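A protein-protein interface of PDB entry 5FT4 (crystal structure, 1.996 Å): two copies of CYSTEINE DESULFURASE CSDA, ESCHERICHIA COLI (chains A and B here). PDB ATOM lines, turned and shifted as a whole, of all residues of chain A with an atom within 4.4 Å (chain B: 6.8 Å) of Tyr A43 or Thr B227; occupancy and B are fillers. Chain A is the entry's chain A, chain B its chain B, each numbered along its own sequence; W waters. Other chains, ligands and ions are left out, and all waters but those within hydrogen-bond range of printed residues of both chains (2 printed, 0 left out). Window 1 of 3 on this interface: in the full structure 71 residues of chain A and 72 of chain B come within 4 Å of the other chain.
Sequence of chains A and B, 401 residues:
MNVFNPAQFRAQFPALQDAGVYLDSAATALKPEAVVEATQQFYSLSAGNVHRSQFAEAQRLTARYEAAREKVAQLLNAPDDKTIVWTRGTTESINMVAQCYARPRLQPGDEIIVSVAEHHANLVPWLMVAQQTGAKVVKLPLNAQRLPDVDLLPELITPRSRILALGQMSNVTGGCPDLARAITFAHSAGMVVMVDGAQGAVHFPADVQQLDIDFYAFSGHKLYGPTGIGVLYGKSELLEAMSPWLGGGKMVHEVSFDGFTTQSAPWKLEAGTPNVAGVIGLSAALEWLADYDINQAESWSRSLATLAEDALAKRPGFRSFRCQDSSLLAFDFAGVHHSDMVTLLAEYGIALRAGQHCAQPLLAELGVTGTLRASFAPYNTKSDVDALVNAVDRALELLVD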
ATOM      1  N   THR A  39       0.953 -13.246   1.387  1.00  0.00           N
ATOM      2  CA  THR A  39      -0.184 -13.358   0.498  1.00  0.00           C
ATOM      3  C   THR A  39      -1.357 -12.451   0.912  1.00  0.00           C
ATOM      4  O   THR A  39      -1.996 -11.820   0.055  1.00  0.00           O
ATOM      5  CB  THR A  39      -0.667 -14.805   0.395  1.00  0.00           C
ATOM      6  OG1 THR A  39       0.415 -15.617  -0.044  1.00  0.00           O
ATOM      7  CG2 THR A  39      -1.817 -14.930  -0.627  1.00  0.00           C
ATOM      8  N   GLN A  40      -1.656 -12.391   2.205  1.00  0.00           N
ATOM      9  CA  GLN A  40      -2.709 -11.517   2.718  1.00  0.00           C
ATOM     10  C   GLN A  40      -2.408 -10.056   2.405  1.00  0.00           C
ATOM     11  O   GLN A  40      -3.282  -9.291   2.006  1.00  0.00           O
ATOM     12  CB  GLN A  40      -2.882 -11.667   4.219  1.00  0.00           C
ATOM     13  CG  GLN A  40      -3.855 -10.682   4.828  1.00  0.00           C
ATOM     14  CD  GLN A  40      -4.657 -11.298   5.939  1.00  0.00           C
ATOM     15  OE1 GLN A  40      -5.528 -12.129   5.696  1.00  0.00           O
ATOM     16  NE2 GLN A  40      -4.361 -10.910   7.169  1.00  0.00           N
ATOM     17  N   GLN A  41      -1.163  -9.668   2.616  1.00  0.00           N
ATOM     18  CA  GLN A  41      -0.766  -8.304   2.338  1.00  0.00           C
ATOM     19  C   GLN A  41      -0.907  -7.978   0.847  1.00  0.00           C
ATOM     20  O   GLN A  41      -1.341  -6.870   0.479  1.00  0.00           O
ATOM     21  CB  GLN A  41       0.656  -8.083   2.804  1.00  0.00           C
ATOM     22  CG  GLN A  41       0.760  -7.996   4.318  1.00  0.00           C
ATOM     23  CD  GLN A  41       2.157  -7.688   4.800  1.00  0.00           C
ATOM     24  OE1 GLN A  41       3.000  -7.228   4.033  1.00  0.00           O
ATOM     25  NE2 GLN A  41       2.393  -7.888   6.092  1.00  0.00           N
ATOM     26  N   PHE A  42      -0.509  -8.924   0.001  1.00  0.00           N
ATOM     27  CA  PHE A  42      -0.559  -8.712  -1.430  1.00  0.00           C
ATOM     28  C   PHE A  42      -1.988  -8.473  -1.917  1.00  0.00           C
ATOM     29  O   PHE A  42      -2.202  -7.636  -2.792  1.00  0.00           O
ATOM     30  CB  PHE A  42       0.052  -9.888  -2.202  1.00  0.00           C
ATOM     31  CG  PHE A  42      -0.145  -9.760  -3.688  1.00  0.00           C
ATOM     32  CD1 PHE A  42       0.505  -8.772  -4.379  1.00  0.00           C
ATOM     33  CD2 PHE A  42      -1.021 -10.582  -4.360  1.00  0.00           C
ATOM     34  CE1 PHE A  42       0.304  -8.602  -5.739  1.00  0.00           C
ATOM     35  CE2 PHE A  42      -1.226 -10.425  -5.728  1.00  0.00           C
ATOM     36  CZ  PHE A  42      -0.576  -9.426  -6.405  1.00  0.00           C
ATOM     37  N   TYR A  43      -2.961  -9.216  -1.388  1.00  0.00           N
ATOM     38  CA  TYR A  43      -4.347  -9.019  -1.792  1.00  0.00           C
ATOM     39  C   TYR A  43      -5.069  -7.867  -1.046  1.00  0.00           C
ATOM     40  O   TYR A  43      -6.203  -7.513  -1.407  1.00  0.00           O
ATOM     41  CB  TYR A  43      -5.122 -10.342  -1.620  1.00  0.00           C
ATOM     42  CG  TYR A  43      -4.805 -11.345  -2.703  1.00  0.00           C
ATOM     43  CD1 TYR A  43      -4.768 -10.962  -4.059  1.00  0.00           C
ATOM     44  CD2 TYR A  43      -4.513 -12.664  -2.393  1.00  0.00           C
ATOM     45  CE1 TYR A  43      -4.487 -11.873  -5.059  1.00  0.00           C
ATOM     46  CE2 TYR A  43      -4.213 -13.594  -3.407  1.00  0.00           C
ATOM     47  CZ  TYR A  43      -4.215 -13.181  -4.734  1.00  0.00           C
ATOM     48  OH  TYR A  43      -3.909 -14.097  -5.713  1.00  0.00           O
ATOM     49  N   SER A  44      -4.417  -7.277  -0.032  1.00  0.00           N
ATOM     50  CA  SER A  44      -5.027  -6.216   0.785  1.00  0.00           C
ATOM     51  C   SER A  44      -4.464  -4.845   0.434  1.00  0.00           C
ATOM     52  O   SER A  44      -4.827  -3.864   1.042  1.00  0.00           O
ATOM     53  CB  SER A  44      -4.810  -6.456   2.272  1.00  0.00           C
ATOM     54  OG  SER A  44      -5.316  -7.700   2.615  1.00  0.00           O
ATOM     55  N   LEU A  45      -3.589  -4.806  -0.560  1.00  0.00           N
ATOM     56  CA  LEU A  45      -2.949  -3.567  -1.005  1.00  0.00           C
ATOM     57  C   LEU A  45      -3.120  -3.338  -2.481  1.00  0.00           C
ATOM     58  O   LEU A  45      -3.137  -4.281  -3.254  1.00  0.00           O
ATOM     59  CB  LEU A  45      -1.445  -3.618  -0.697  1.00  0.00           C
ATOM     60  CG  LEU A  45      -0.974  -3.365   0.712  1.00  0.00           C
ATOM     61  CD1 LEU A  45       0.538  -3.444   0.778  1.00  0.00           C
ATOM     62  CD2 LEU A  45      -1.439  -1.992   1.131  1.00  0.00           C
ATOM     63  N   PRO A 274       1.837 -12.461 -14.990  1.00  0.00           N
ATOM     64  CA  PRO A 274       2.358 -13.533 -14.130  1.00  0.00           C
ATOM     65  C   PRO A 274       1.386 -13.860 -12.978  1.00  0.00           C
ATOM     66  O   PRO A 274       0.459 -13.085 -12.656  1.00  0.00           O
ATOM     67  CB  PRO A 274       3.664 -12.939 -13.560  1.00  0.00           C
ATOM     68  CG  PRO A 274       3.939 -11.693 -14.304  1.00  0.00           C
ATOM     69  CD  PRO A 274       2.617 -11.215 -14.849  1.00  0.00           C
ATOM     70  N   ASN A 275       1.585 -15.009 -12.361  1.00  0.00           N
ATOM     71  CA  ASN A 275       0.875 -15.286 -11.141  1.00  0.00           C
ATOM     72  C   ASN A 275       1.639 -14.571 -10.040  1.00  0.00           C
ATOM     73  O   ASN A 275       2.394 -15.194  -9.312  1.00  0.00           O
ATOM     74  CB  ASN A 275       0.747 -16.787 -10.881  1.00  0.00           C
ATOM     75  CG  ASN A 275       0.136 -17.073  -9.520  1.00  0.00           C
ATOM     76  OD1 ASN A 275      -0.345 -16.156  -8.838  1.00  0.00           O
ATOM     77  ND2 ASN A 275       0.185 -18.322  -9.095  1.00  0.00           N
ATOM     78  N   VAL A 276       1.423 -13.253  -9.940  1.00  0.00           N
ATOM     79  CA  VAL A 276       2.174 -12.387  -9.049  1.00  0.00           C
ATOM     80  C   VAL A 276       2.050 -12.846  -7.592  1.00  0.00           C
ATOM     81  O   VAL A 276       3.030 -12.827  -6.847  1.00  0.00           O
ATOM     82  CB  VAL A 276       1.712 -10.908  -9.204  1.00  0.00           C
ATOM     83  CG1 VAL A 276       2.395  -9.988  -8.207  1.00  0.00           C
ATOM     84  CG2 VAL A 276       1.975 -10.402 -10.619  1.00  0.00           C
ATOM     85  N   ALA A 277       0.855 -13.258  -7.175  1.00  0.00           N
ATOM     86  CA  ALA A 277       0.676 -13.773  -5.810  1.00  0.00           C
ATOM     87  C   ALA A 277       1.556 -15.009  -5.556  1.00  0.00           C
ATOM     88  O   ALA A 277       2.172 -15.165  -4.473  1.00  0.00           O
ATOM     89  CB  ALA A 277      -0.792 -14.129  -5.569  1.00  0.00           C
ATOM     90  N   PRO B  14     -10.483  -3.782   1.183  1.00  0.00           N
ATOM     91  CA  PRO B  14      -9.553  -3.263   2.196  1.00  0.00           C
ATOM     92  C   PRO B  14      -8.441  -2.365   1.652  1.00  0.00           C
ATOM     93  O   PRO B  14      -7.917  -1.563   2.418  1.00  0.00           O
ATOM     94  CB  PRO B  14      -8.956  -4.535   2.803  1.00  0.00           C
ATOM     95  CG  PRO B  14      -9.098  -5.558   1.741  1.00  0.00           C
ATOM     96  CD  PRO B  14     -10.389  -5.245   1.058  1.00  0.00           C
ATOM     97  N   ALA B  15      -8.104  -2.497   0.373  1.00  0.00           N
ATOM     98  CA  ALA B  15      -7.040  -1.714  -0.261  1.00  0.00           C
ATOM     99  C   ALA B  15      -7.419  -0.248  -0.546  1.00  0.00           C
ATOM    100  O   ALA B  15      -6.558   0.569  -0.894  1.00  0.00           O
ATOM    101  CB  ALA B  15      -6.608  -2.407  -1.599  1.00  0.00           C
ATOM    102  N   THR B  28      -5.642  -4.380 -13.590  1.00  0.00           N
ATOM    103  CA  THR B  28      -5.935  -5.370 -12.555  1.00  0.00           C
ATOM    104  C   THR B  28      -6.847  -4.735 -11.481  1.00  0.00           C
ATOM    105  O   THR B  28      -6.710  -3.550 -11.170  1.00  0.00           O
ATOM    106  CB  THR B  28      -4.608  -5.924 -11.940  1.00  0.00           C
ATOM    107  OG1 THR B  28      -4.804  -7.236 -11.422  1.00  0.00           O
ATOM    108  CG2 THR B  28      -4.052  -5.012 -10.839  1.00  0.00           C
ATOM    109  N   LEU B  30      -8.850  -4.302  -7.714  1.00  0.00           N
ATOM    110  CA  LEU B  30      -8.717  -4.494  -6.258  1.00  0.00           C
ATOM    111  C   LEU B  30      -9.595  -5.661  -5.850  1.00  0.00           C
ATOM    112  O   LEU B  30     -10.508  -6.021  -6.605  1.00  0.00           O
ATOM    113  CB  LEU B  30      -9.109  -3.236  -5.497  1.00  0.00           C
ATOM    114  CG  LEU B  30      -8.353  -1.951  -5.915  1.00  0.00           C
ATOM    115  CD1 LEU B  30      -8.830  -0.779  -5.107  1.00  0.00           C
ATOM    116  CD2 LEU B  30      -6.845  -2.139  -5.762  1.00  0.00           C
ATOM    117  N   LYS B  31      -9.333  -6.257  -4.682  1.00  0.00           N
ATOM    118  CA  LYS B  31     -10.052  -7.468  -4.242  1.00  0.00           C
ATOM    119  C   LYS B  31     -10.972  -7.188  -3.064  1.00  0.00           C
ATOM    120  O   LYS B  31     -10.595  -6.469  -2.156  1.00  0.00           O
ATOM    121  CB  LYS B  31      -9.110  -8.596  -3.812  1.00  0.00           C
ATOM    122  CG  LYS B  31      -7.815  -8.769  -4.631  1.00  0.00           C
ATOM    123  CD  LYS B  31      -8.041  -8.790  -6.138  1.00  0.00           C
ATOM    124  CE  LYS B  31      -6.692  -8.983  -6.864  1.00  0.00           C
ATOM    125  NZ  LYS B  31      -6.850  -8.818  -8.309  1.00  0.00           N
ATOM    126  N   PRO B  32     -12.170  -7.784  -3.067  1.00  0.00           N
ATOM    127  CA  PRO B  32     -13.044  -7.706  -1.889  1.00  0.00           C
ATOM    128  C   PRO B  32     -12.544  -8.576  -0.734  1.00  0.00           C
ATOM    129  O   PRO B  32     -11.791  -9.522  -0.983  1.00  0.00           O
ATOM    130  CB  PRO B  32     -14.374  -8.244  -2.405  1.00  0.00           C
ATOM    131  CG  PRO B  32     -13.972  -9.249  -3.442  1.00  0.00           C
ATOM    132  CD  PRO B  32     -12.734  -8.653  -4.116  1.00  0.00           C
ATOM    133  N   VAL B  35     -12.337 -12.506  -0.894  1.00  0.00           N
ATOM    134  CA  VAL B  35     -11.184 -13.111  -1.569  1.00  0.00           C
ATOM    135  C   VAL B  35      -9.959 -13.179  -0.672  1.00  0.00           C
ATOM    136  O   VAL B  35      -9.261 -14.191  -0.619  1.00  0.00           O
ATOM    137  CB  VAL B  35     -10.791 -12.327  -2.851  1.00  0.00           C
ATOM    138  CG1 VAL B  35      -9.427 -12.804  -3.409  1.00  0.00           C
ATOM    139  CG2 VAL B  35     -11.873 -12.456  -3.863  1.00  0.00           C
ATOM    140  N   VAL B  36      -9.691 -12.095   0.038  1.00  0.00           N
ATOM    141  CA  VAL B  36      -8.562 -12.066   0.960  1.00  0.00           C
ATOM    142  C   VAL B  36      -8.722 -13.145   2.035  1.00  0.00           C
ATOM    143  O   VAL B  36      -7.781 -13.897   2.360  1.00  0.00           O
ATOM    144  CB  VAL B  36      -8.430 -10.699   1.632  1.00  0.00           C
ATOM    145  CG1 VAL B  36      -7.239 -10.690   2.602  1.00  0.00           C
ATOM    146  CG2 VAL B  36      -8.311  -9.578   0.565  1.00  0.00           C
ATOM    147  N   THR B  39      -8.603 -16.886   0.902  1.00  0.00           N
ATOM    148  CA  THR B  39      -7.218 -17.246   0.597  1.00  0.00           C
ATOM    149  C   THR B  39      -6.405 -17.474   1.881  1.00  0.00           C
ATOM    150  O   THR B  39      -5.600 -18.412   1.979  1.00  0.00           O
ATOM    151  CB  THR B  39      -6.552 -16.167  -0.278  1.00  0.00           C
ATOM    152  OG1 THR B  39      -7.307 -16.005  -1.490  1.00  0.00           O
ATOM    153  CG2 THR B  39      -5.125 -16.549  -0.654  1.00  0.00           C
ATOM    154  N   TYR B  43      -4.682 -21.177   3.081  1.00  0.00           N
ATOM    155  CA  TYR B  43      -3.268 -21.373   3.357  1.00  0.00           C
ATOM    156  C   TYR B  43      -2.959 -21.635   4.835  1.00  0.00           C
ATOM    157  O   TYR B  43      -1.813 -21.950   5.180  1.00  0.00           O
ATOM    158  CB  TYR B  43      -2.476 -20.182   2.836  1.00  0.00           C
ATOM    159  CG  TYR B  43      -2.230 -20.178   1.311  1.00  0.00           C
ATOM    160  CD1 TYR B  43      -1.809 -21.330   0.656  1.00  0.00           C
ATOM    161  CD2 TYR B  43      -2.423 -19.027   0.534  1.00  0.00           C
ATOM    162  CE1 TYR B  43      -1.543 -21.354  -0.720  1.00  0.00           C
ATOM    163  CE2 TYR B  43      -2.156 -19.043  -0.865  1.00  0.00           C
ATOM    164  CZ  TYR B  43      -1.716 -20.228  -1.471  1.00  0.00           C
ATOM    165  OH  TYR B  43      -1.440 -20.317  -2.819  1.00  0.00           O
ATOM    166  N   ARG B  88      -4.506 -20.472 -16.481  1.00  0.00           N
ATOM    167  CA  ARG B  88      -3.799 -19.517 -15.651  1.00  0.00           C
ATOM    168  C   ARG B  88      -4.147 -18.096 -16.075  1.00  0.00           C
ATOM    169  O   ARG B  88      -3.698 -17.131 -15.449  1.00  0.00           O
ATOM    170  CB  ARG B  88      -2.279 -19.753 -15.702  1.00  0.00           C
ATOM    171  CG  ARG B  88      -1.598 -19.481 -17.012  1.00  0.00           C
ATOM    172  CD  ARG B  88      -0.090 -19.588 -16.815  1.00  0.00           C
ATOM    173  NE  ARG B  88       0.684 -19.238 -18.000  1.00  0.00           N
ATOM    174  CZ  ARG B  88       0.792 -18.011 -18.501  1.00  0.00           C
ATOM    175  NH1 ARG B  88       0.154 -16.987 -17.944  1.00  0.00           N
ATOM    176  NH2 ARG B  88       1.536 -17.807 -19.579  1.00  0.00           N
ATOM    177  N   GLY B 220      -9.063 -14.049 -13.932  1.00  0.00           N
ATOM    178  CA  GLY B 220      -9.572 -13.827 -12.591  1.00  0.00           C
ATOM    179  C   GLY B 220      -9.152 -12.499 -11.986  1.00  0.00           C
ATOM    180  O   GLY B 220      -9.923 -11.890 -11.227  1.00  0.00           O
ATOM    181  N   HIS B 221      -7.939 -12.042 -12.288  1.00  0.00           N
ATOM    182  CA  HIS B 221      -7.368 -10.895 -11.545  1.00  0.00           C
ATOM    183  C   HIS B 221      -8.029  -9.549 -11.934  1.00  0.00           C
ATOM    184  O   HIS B 221      -8.019  -8.597 -11.150  1.00  0.00           O
ATOM    185  CB  HIS B 221      -5.837 -10.863 -11.712  1.00  0.00           C
ATOM    186  CG  HIS B 221      -5.349 -10.521 -13.090  1.00  0.00           C
ATOM    187  ND1 HIS B 221      -5.044  -9.235 -13.472  1.00  0.00           N
ATOM    188  CD2 HIS B 221      -5.061 -11.311 -14.162  1.00  0.00           C
ATOM    189  CE1 HIS B 221      -4.613  -9.236 -14.726  1.00  0.00           C
ATOM    190  NE2 HIS B 221      -4.630 -10.484 -15.172  1.00  0.00           N
ATOM    191  N   GLY B 225     -10.411 -10.795  -8.534  1.00  0.00           N
ATOM    192  CA  GLY B 225     -10.012 -12.092  -8.028  1.00  0.00           C
ATOM    193  C   GLY B 225      -8.511 -12.350  -8.019  1.00  0.00           C
ATOM    194  O   GLY B 225      -7.724 -11.475  -8.295  1.00  0.00           O
ATOM    195  N   PRO B 226      -8.129 -13.589  -7.713  1.00  0.00           N
ATOM    196  CA  PRO B 226      -6.731 -13.967  -7.575  1.00  0.00           C
ATOM    197  C   PRO B 226      -5.950 -13.857  -8.853  1.00  0.00           C
ATOM    198  O   PRO B 226      -6.545 -13.898  -9.923  1.00  0.00           O
ATOM    199  CB  PRO B 226      -6.798 -15.439  -7.150  1.00  0.00           C
ATOM    200  CG  PRO B 226      -8.167 -15.624  -6.603  1.00  0.00           C
ATOM    201  CD  PRO B 226      -9.037 -14.712  -7.409  1.00  0.00           C
ATOM    202  N   THR B 227      -4.635 -13.745  -8.734  1.00  0.00           N
ATOM    203  CA  THR B 227      -3.760 -13.888  -9.903  1.00  0.00           C
ATOM    204  C   THR B 227      -3.577 -15.368 -10.197  1.00  0.00           C
ATOM    205  O   THR B 227      -3.901 -16.235  -9.351  1.00  0.00           O
ATOM    206  CB  THR B 227      -2.382 -13.200  -9.688  1.00  0.00           C
ATOM    207  OG1 THR B 227      -1.752 -13.706  -8.516  1.00  0.00           O
ATOM    208  CG2 THR B 227      -2.526 -11.669  -9.541  1.00  0.00           C
ATOM    209  N   GLY B 228      -3.069 -15.664 -11.389  1.00  0.00           N
ATOM    210  CA  GLY B 228      -2.704 -17.031 -11.746  1.00  0.00           C
ATOM    211  C   GLY B 228      -3.877 -17.954 -12.016  1.00  0.00           C
ATOM    212  O   GLY B 228      -3.746 -19.191 -11.968  1.00  0.00           O
ATOM    213  N   ILE B 229      -5.041 -17.376 -12.276  1.00  0.00           N
ATOM    214  CA  ILE B 229      -6.224 -18.187 -12.584  1.00  0.00           C
ATOM    215  C   ILE B 229      -7.027 -17.516 -13.704  1.00  0.00           C
ATOM    216  O   ILE B 229      -7.218 -16.293 -13.734  1.00  0.00           O
ATOM    217  CB  ILE B 229      -7.125 -18.400 -11.324  1.00  0.00           C
ATOM    218  CG1 ILE B 229      -8.189 -19.478 -11.572  1.00  0.00           C
ATOM    219  CG2 ILE B 229      -7.800 -17.120 -10.875  1.00  0.00           C
ATOM    220  CD1 ILE B 229      -7.595 -20.872 -11.723  1.00  0.00           C
ATOM    221  N   GLY B 230      -7.480 -18.341 -14.634  1.00  0.00           N
ATOM    222  CA  GLY B 230      -8.371 -17.894 -15.692  1.00  0.00           C
ATOM    223  C   GLY B 230      -9.365 -18.981 -16.083  1.00  0.00           C
ATOM    224  O   GLY B 230      -9.324 -20.105 -15.580  1.00  0.00           O
ATOM    225  N   ASN B 275      -4.283 -24.794  -9.509  1.00  0.00           N
ATOM    226  CA  ASN B 275      -4.019 -23.645  -8.681  1.00  0.00           C
ATOM    227  C   ASN B 275      -5.195 -23.558  -7.728  1.00  0.00           C
ATOM    228  O   ASN B 275      -6.116 -22.755  -7.924  1.00  0.00           O
ATOM    229  CB  ASN B 275      -3.867 -22.363  -9.497  1.00  0.00           C
ATOM    230  CG  ASN B 275      -3.603 -21.166  -8.617  1.00  0.00           C
ATOM    231  OD1 ASN B 275      -3.392 -21.311  -7.388  1.00  0.00           O
ATOM    232  ND2 ASN B 275      -3.533 -19.983  -9.232  1.00  0.00           N
ATOM    233  N   ALA B 277      -5.625 -22.457  -4.709  1.00  0.00           N
ATOM    234  CA  ALA B 277      -5.881 -21.135  -4.063  1.00  0.00           C
ATOM    235  C   ALA B 277      -6.581 -20.176  -5.024  1.00  0.00           C
ATOM    236  O   ALA B 277      -7.445 -19.396  -4.632  1.00  0.00           O
ATOM    237  CB  ALA B 277      -4.611 -20.519  -3.593  1.00  0.00           C
ATOM    238  N   GLY B 278      -6.142 -20.212  -6.274  1.00  0.00           N
ATOM    239  CA  GLY B 278      -6.737 -19.431  -7.331  1.00  0.00           C
ATOM    240  C   GLY B 278      -8.198 -19.798  -7.570  1.00  0.00           C
ATOM    241  O   GLY B 278      -9.014 -18.917  -7.693  1.00  0.00           O
HETATM  242  O   HOH W   1      -6.992  -5.477  -3.202  1.00  0.00           O
HETATM  243  O   HOH W   2      -2.385 -13.668 -13.127  1.00  0.00           O
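The backbone NH of Thr B227 is in hydrogen-bond range of the side-chain hydroxyl of Tyr A43, at 3.1 Å. The side-chain amide oxygen of Asn A275 lies within hydrogen-bond range of the side-chain hydroxyl of Thr B227 (2.8 Å). The backbone NH of Ala A277 lies within hydrogen-bond range of the side-chain hydroxyl of Thr B227 (3.0 Å).
Of the 22 printed residues of chain B, 8 touch a printed residue of chain A. Printed residues of chain B that touch a printed residue of chain A: Pro B14, Ala B15, Lys B31, Val B36, Thr B39, Pro B226, Thr B227 and Gly B228. Along chain B the printed residues that touch a printed residue of chain A span positions 14 to 228. Among the printed residues, 14 pairs touch across the chains. Among the printed residues, no Asp or Glu carboxylate lies within 4 Å of a Lys or Arg side-chain nitrogen of the other chain.
Thr A39 touches its own counterpart, Thr B39. 4 positions are printed for both chains. Of the 14 pairs that touch across the chains among the printed residues, 1 has its exchanged pair printed and touching as well.
Gln A41 touches none of the printed residues of chain B. Of chain B, only Lys B31, Val B36, Pro B226 and Thr B227 come within 4 Å of Tyr A43. Of the printed residues of chain B, Val A276 touches Thr B227 (3.5 Å). Of the printed residues of chain A, Ala B15 touches Ser A44 (3.3 Å) and Leu A45 (3.7 Å). Thr B28 touches none of the printed residues of chain A. Of the printed residues of chain A, Lys B31 touches Tyr A43. Printed residues of chain A within 4 Å of Val B36: Gln A40, Tyr A43 and Ser A44. Thr B227 touches four residues of chain A. The nearest residue of chain A that does not touch Thr B227 is Pro A274 (4.1 Å). The nearest printed residue of chain B that does not touch Thr A39 is Tyr B43 (4.1 Å).
Thr A39 touches Thr B39 (CG2 to CG2, 3.7 Å). Gln A40 touches Val B36. Tyr A43 touches Lys B31 (CD1 to CG, 3.8 Å). Val B36 touches Tyr A43. OH of Tyr A43 touches CA of Pro B226, at 3.4 Å. Ser A44 touches Pro B14 (O to C, 3.96 Å). O of Ser A44 touches CA of Ala B15, 3.3 Å away. Ser A44 touches Val B36. C of Leu A45 touches CB of Ala B15, 3.7 Å away. OG1 of Thr B227 touches N of Val A276 (3.5 Å).
The backbone carbonyl oxygen (O) of Gln A40 lies within hydrogen-bond range of the side-chain hydroxyl (OG) of Ser A44 (2.7 Å). The backbone carbonyl oxygen of His B221 is in hydrogen-bond range of the side-chain amino group of Lys B31 (3.1 Å). The backbone carbonyl oxygen (O) of Gly B225 is in hydrogen-bond range of the side-chain amino group (NZ) of Lys B31 (2.8 Å). The backbone carbonyl oxygen of Val B35 lies within hydrogen-bond range of the side-chain hydroxyl of Thr B39, 2.8 Å away. The backbone NH (N) of His B221 sits at hydrogen-bond distance from the backbone carbonyl oxygen (O) of Pro B226, at 3.3 Å. ND2 of Asn B275 is in hydrogen-bond range of O of Gly B228 (2.9 Å).
Water W2 lies within hydrogen-bond range of the backbone NH (N) of Gly B228 (2.7 Å) and the backbone carbonyl oxygen (O) of Pro A274 (2.9 Å). Water W1 lies within hydrogen-bond range of O of Tyr A43 (2.8 Å) and N of Lys B31 (2.9 Å).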
